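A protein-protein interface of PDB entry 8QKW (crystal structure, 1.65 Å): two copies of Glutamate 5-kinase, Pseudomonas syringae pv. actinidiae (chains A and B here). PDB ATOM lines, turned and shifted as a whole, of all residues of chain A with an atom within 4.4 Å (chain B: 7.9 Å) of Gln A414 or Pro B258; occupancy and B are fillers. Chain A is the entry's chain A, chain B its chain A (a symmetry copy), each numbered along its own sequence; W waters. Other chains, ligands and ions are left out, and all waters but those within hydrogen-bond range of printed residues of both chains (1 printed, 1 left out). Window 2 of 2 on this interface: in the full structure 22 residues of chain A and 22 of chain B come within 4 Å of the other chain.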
ATOM      1  N   VAL A 402      37.493  12.959 -17.013  1.00  0.00           N
ATOM      2  CA  VAL A 402      36.422  13.299 -16.066  1.00  0.00           C
ATOM      3  C   VAL A 402      36.462  12.262 -14.927  1.00  0.00           C
ATOM      4  O   VAL A 402      36.797  11.117 -15.149  1.00  0.00           O
ATOM      5  CB  VAL A 402      35.038  13.331 -16.780  1.00  0.00           C
ATOM      6  CG1 VAL A 402      34.607  11.965 -17.298  1.00  0.00           C
ATOM      7  CG2 VAL A 402      33.919  13.910 -15.907  1.00  0.00           C
ATOM      8  N   ARG A 403      36.115  12.657 -13.687  1.00  0.00           N
ATOM      9  CA  ARG A 403      36.105  11.728 -12.576  1.00  0.00           C
ATOM     10  C   ARG A 403      34.684  11.202 -12.400  1.00  0.00           C
ATOM     11  O   ARG A 403      33.734  11.958 -12.619  1.00  0.00           O
ATOM     12  CB  ARG A 403      36.536  12.422 -11.279  1.00  0.00           C
ATOM     13  CG  ARG A 403      36.652  11.440 -10.112  1.00  0.00           C
ATOM     14  CD  ARG A 403      37.353  12.092  -8.888  1.00  0.00           C
ATOM     15  NE  ARG A 403      36.562  13.206  -8.370  1.00  0.00           N
ATOM     16  CZ  ARG A 403      35.631  13.087  -7.410  1.00  0.00           C
ATOM     17  NH1 ARG A 403      35.490  11.931  -6.768  1.00  0.00           N
ATOM     18  NH2 ARG A 403      34.903  14.135  -7.031  1.00  0.00           N
ATOM     19  N   VAL A 405      32.385   8.790  -9.453  1.00  0.00           N
ATOM     20  CA  VAL A 405      32.464   8.058  -8.197  1.00  0.00           C
ATOM     21  C   VAL A 405      31.473   6.899  -8.237  1.00  0.00           C
ATOM     22  O   VAL A 405      30.416   6.970  -8.873  1.00  0.00           O
ATOM     23  CB  VAL A 405      32.246   8.969  -6.976  1.00  0.00           C
ATOM     24  CG1 VAL A 405      33.414   9.905  -6.712  1.00  0.00           C
ATOM     25  CG2 VAL A 405      30.942   9.727  -7.088  1.00  0.00           C
ATOM     26  N   PHE A 412      28.306   8.144 -10.528  1.00  0.00           N
ATOM     27  CA  PHE A 412      27.930   9.570 -10.580  1.00  0.00           C
ATOM     28  C   PHE A 412      29.109  10.326 -11.194  1.00  0.00           C
ATOM     29  O   PHE A 412      30.224  10.260 -10.675  1.00  0.00           O
ATOM     30  CB  PHE A 412      27.720  10.112  -9.148  1.00  0.00           C
ATOM     31  CG  PHE A 412      26.586   9.435  -8.420  1.00  0.00           C
ATOM     32  CD1 PHE A 412      26.781   8.286  -7.672  1.00  0.00           C
ATOM     33  CD2 PHE A 412      25.287   9.983  -8.520  1.00  0.00           C
ATOM     34  CE1 PHE A 412      25.716   7.669  -6.999  1.00  0.00           C
ATOM     35  CE2 PHE A 412      24.233   9.383  -7.836  1.00  0.00           C
ATOM     36  CZ  PHE A 412      24.449   8.221  -7.089  1.00  0.00           C
ATOM     37  N   VAL A 413      28.839  11.080 -12.276  1.00  0.00           N
ATOM     38  CA  VAL A 413      29.897  11.886 -12.889  1.00  0.00           C
ATOM     39  C   VAL A 413      30.198  13.111 -12.025  1.00  0.00           C
ATOM     40  O   VAL A 413      29.306  13.693 -11.397  1.00  0.00           O
ATOM     41  CB  VAL A 413      29.548  12.254 -14.336  1.00  0.00           C
ATOM     42  CG1 VAL A 413      28.458  13.319 -14.388  1.00  0.00           C
ATOM     43  CG2 VAL A 413      30.823  12.732 -15.097  1.00  0.00           C
ATOM     44  N   GLN A 414      31.500  13.455 -11.976  1.00  0.00           N
ATOM     45  CA  GLN A 414      31.978  14.544 -11.135  1.00  0.00           C
ATOM     46  C   GLN A 414      32.778  15.499 -12.036  1.00  0.00           C
ATOM     47  O   GLN A 414      32.353  15.762 -13.156  1.00  0.00           O
ATOM     48  CB  GLN A 414      32.750  13.978  -9.930  1.00  0.00           C
ATOM     49  CG  GLN A 414      31.936  13.057  -9.003  1.00  0.00           C
ATOM     50  CD  GLN A 414      30.985  13.875  -8.158  1.00  0.00           C
ATOM     51  OE1 GLN A 414      29.862  14.211  -8.550  1.00  0.00           O
ATOM     52  NE2 GLN A 414      31.464  14.270  -6.994  1.00  0.00           N
ATOM     53  N   GLU A 415      33.858  16.095 -11.497  1.00  0.00           N
ATOM     54  CA  GLU A 415      34.398  17.240 -12.223  1.00  0.00           C
ATOM     55  C   GLU A 415      35.286  16.781 -13.375  1.00  0.00           C
ATOM     56  O   GLU A 415      35.795  15.649 -13.407  1.00  0.00           O
ATOM     57  CB  GLU A 415      35.248  18.098 -11.265  1.00  0.00           C
ATOM     58  CG  GLU A 415      36.464  17.381 -10.709  1.00  0.00           C
ATOM     59  CD  GLU A 415      36.296  16.366  -9.576  1.00  0.00           C
ATOM     60  OE1 GLU A 415      35.172  16.277  -9.010  1.00  0.00           O
ATOM     61  OE2 GLU A 415      37.230  15.623  -9.304  1.00  0.00           O
ATOM     62  N   GLU A 416      35.575  17.747 -14.239  1.00  0.00           N
ATOM     63  CA  GLU A 416      36.371  17.485 -15.423  1.00  0.00           C
ATOM     64  C   GLU A 416      37.756  18.088 -15.261  1.00  0.00           C
ATOM     65  O   GLU A 416      37.956  19.011 -14.450  1.00  0.00           O
ATOM     66  CB  GLU A 416      35.593  17.843 -16.688  1.00  0.00           C
ATOM     67  CG  GLU A 416      35.840  19.162 -17.315  1.00  0.00           C
ATOM     68  CD  GLU A 416      34.999  19.362 -18.570  1.00  0.00           C
ATOM     69  OE1 GLU A 416      35.550  19.228 -19.685  1.00  0.00           O
ATOM     70  OE2 GLU A 416      33.788  19.723 -18.431  1.00  0.00           O
ATOM     71  N   ALA B  30      21.386  13.663  -5.597  1.00  0.00           N
ATOM     72  CA  ALA B  30      22.012  12.990  -6.747  1.00  0.00           C
ATOM     73  C   ALA B  30      21.245  11.733  -7.155  1.00  0.00           C
ATOM     74  O   ALA B  30      21.163  11.438  -8.355  1.00  0.00           O
ATOM     75  CB  ALA B  30      23.447  12.596  -6.361  1.00  0.00           C
ATOM     76  N   LEU B  33      18.273  12.861  -9.149  1.00  0.00           N
ATOM     77  CA  LEU B  33      18.617  13.332 -10.508  1.00  0.00           C
ATOM     78  C   LEU B  33      18.538  12.205 -11.532  1.00  0.00           C
ATOM     79  O   LEU B  33      18.447  12.480 -12.749  1.00  0.00           O
ATOM     80  CB  LEU B  33      19.994  14.025 -10.576  1.00  0.00           C
ATOM     81  CG  LEU B  33      20.044  15.399  -9.898  1.00  0.00           C
ATOM     82  CD1 LEU B  33      21.495  15.900  -9.843  1.00  0.00           C
ATOM     83  CD2 LEU B  33      19.138  16.414 -10.628  1.00  0.00           C
ATOM     84  N   GLY B 254      24.366  14.540  -1.962  1.00  0.00           N
ATOM     85  CA  GLY B 254      24.970  13.407  -2.663  1.00  0.00           C
ATOM     86  C   GLY B 254      25.927  13.898  -3.766  1.00  0.00           C
ATOM     87  O   GLY B 254      26.220  15.090  -3.892  1.00  0.00           O
ATOM     88  N   PRO B 255      26.474  12.972  -4.584  1.00  0.00           N
ATOM     89  CA  PRO B 255      27.465  13.330  -5.601  1.00  0.00           C
ATOM     90  C   PRO B 255      26.794  13.880  -6.855  1.00  0.00           C
ATOM     91  O   PRO B 255      26.755  13.222  -7.888  1.00  0.00           O
ATOM     92  CB  PRO B 255      28.243  12.008  -5.835  1.00  0.00           C
ATOM     93  CG  PRO B 255      27.391  10.926  -5.223  1.00  0.00           C
ATOM     94  CD  PRO B 255      26.317  11.507  -4.342  1.00  0.00           C
ATOM     95  N   VAL B 256      26.237  15.093  -6.742  1.00  0.00           N
ATOM     96  CA  VAL B 256      25.602  15.714  -7.914  1.00  0.00           C
ATOM     97  C   VAL B 256      26.659  16.129  -8.938  1.00  0.00           C
ATOM     98  O   VAL B 256      27.816  16.387  -8.605  1.00  0.00           O
ATOM     99  CB  VAL B 256      24.737  16.932  -7.534  1.00  0.00           C
ATOM    100  CG1 VAL B 256      23.563  16.477  -6.654  1.00  0.00           C
ATOM    101  CG2 VAL B 256      25.508  18.062  -6.836  1.00  0.00           C
ATOM    102  N   PRO B 257      26.264  16.198 -10.220  1.00  0.00           N
ATOM    103  CA  PRO B 257      27.212  16.588 -11.260  1.00  0.00           C
ATOM    104  C   PRO B 257      27.458  18.086 -11.246  1.00  0.00           C
ATOM    105  O   PRO B 257      26.760  18.863 -10.580  1.00  0.00           O
ATOM    106  CB  PRO B 257      26.528  16.206 -12.563  1.00  0.00           C
ATOM    107  CG  PRO B 257      25.082  15.902 -12.221  1.00  0.00           C
ATOM    108  CD  PRO B 257      24.932  15.848 -10.718  1.00  0.00           C
ATOM    109  N   PRO B 258      28.512  18.546 -11.947  1.00  0.00           N
ATOM    110  CA  PRO B 258      28.780  19.981 -12.013  1.00  0.00           C
ATOM    111  C   PRO B 258      27.554  20.736 -12.491  1.00  0.00           C
ATOM    112  O   PRO B 258      26.857  20.294 -13.388  1.00  0.00           O
ATOM    113  CB  PRO B 258      29.908  19.987 -13.081  1.00  0.00           C
ATOM    114  CG  PRO B 258      30.686  18.704 -12.716  1.00  0.00           C
ATOM    115  CD  PRO B 258      29.525  17.713 -12.654  1.00  0.00           C
ATOM    116  N   GLY B 259      27.326  21.887 -11.855  1.00  0.00           N
ATOM    117  CA  GLY B 259      26.229  22.749 -12.239  1.00  0.00           C
ATOM    118  C   GLY B 259      24.999  22.503 -11.370  1.00  0.00           C
ATOM    119  O   GLY B 259      24.021  23.245 -11.477  1.00  0.00           O
ATOM    120  N   HIS B 260      25.027  21.426 -10.563  1.00  0.00           N
ATOM    121  CA  HIS B 260      23.833  21.057  -9.791  1.00  0.00           C
ATOM    122  C   HIS B 260      24.000  21.313  -8.295  1.00  0.00           C
ATOM    123  O   HIS B 260      23.303  20.732  -7.448  1.00  0.00           O
ATOM    124  CB  HIS B 260      23.512  19.587 -10.056  1.00  0.00           C
ATOM    125  CG  HIS B 260      22.778  19.407 -11.329  1.00  0.00           C
ATOM    126  ND1 HIS B 260      23.412  19.309 -12.556  1.00  0.00           N
ATOM    127  CD2 HIS B 260      21.470  19.425 -11.565  1.00  0.00           C
ATOM    128  CE1 HIS B 260      22.486  19.149 -13.487  1.00  0.00           C
ATOM    129  NE2 HIS B 260      21.296  19.277 -12.911  1.00  0.00           N
ATOM    130  N   GLU B 261      24.864  22.251  -7.937  1.00  0.00           N
ATOM    131  CA  GLU B 261      25.220  22.418  -6.527  1.00  0.00           C
ATOM    132  C   GLU B 261      24.268  23.370  -5.788  1.00  0.00           C
ATOM    133  O   GLU B 261      24.247  23.378  -4.567  1.00  0.00           O
ATOM    134  CB  GLU B 261      26.611  23.040  -6.343  1.00  0.00           C
ATOM    135  CG  GLU B 261      27.723  22.232  -6.991  1.00  0.00           C
ATOM    136  CD  GLU B 261      27.976  22.452  -8.477  1.00  0.00           C
ATOM    137  OE1 GLU B 261      27.232  23.259  -9.130  1.00  0.00           O
ATOM    138  OE2 GLU B 261      28.932  21.810  -8.992  1.00  0.00           O
HETATM  139  O   HOH W   1      26.615  12.956 -10.797  1.00  0.00           O
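N of Val A405 sits at hydrogen-bond distance from O of Phe A412.
The backbone carbonyl oxygen (O) of Arg A403 is in hydrogen-bond range of the backbone NH (N) of Gln A414 (2.8 Å).
Hydrophobic or aromatic side chains of chain A that line the printed part of chain B: Val A405, Phe A412 and Val A413.
Among the printed residues, 7 pairs touch across the chains.
Among the printed residues, no Asp or Glu carboxylate lies within 4 Å of a Lys or Arg side-chain nitrogen of the other chain.
OE1 of Gln A414 sits close to O of Val B256 (3.0 Å).
O of Pro B255 lies close to OE1 of Gln A414 (3.3 Å).
Val A405 touches Pro B255.
Phe A412 touches Ala B30 (CE2 to CB, 3.6 Å).
Pro B255 touches Phe A412 (O to CB, 3.5 Å).
Pro B257 touches Val A413.
Gln A414 touches Pro B258.
No position is printed for both chains.
Of the 7 pairs that touch across the chains among the printed residues, none has its exchanged pair printed and touching as well.
Of chain B, only Pro B255 (3.3 Å), Val B256 (3.0 Å) and Pro B258 (3.4 Å) come within 4 Å of Gln A414.
Pro B258 touches just one residue of chain A: Gln A414 (3.4 Å).
Printed residues of chain A within 4 Å of Ala B30: Phe A412.
Printed residues of chain B within 4 Å of Val A405: Pro B255 (3.7 Å).
Of the printed residues of chain A, Val B256 touches Gln A414 (3.0 Å).
Printed residues of chain A within 4 Å of Pro B257: Val A413 (3.6 Å).
Val A402 touches none of the printed residues of chain B.
The nearest residue of chain B that does not touch Gln A414 is Pro B257 (4.4 Å).
The nearest printed residue of chain A that does not touch Pro B257 is Gln A414 (4.4 Å).
Water W1 lies within hydrogen-bond range of O of Val A413 (2.9 Å) and O of Pro B255 (2.9 Å).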
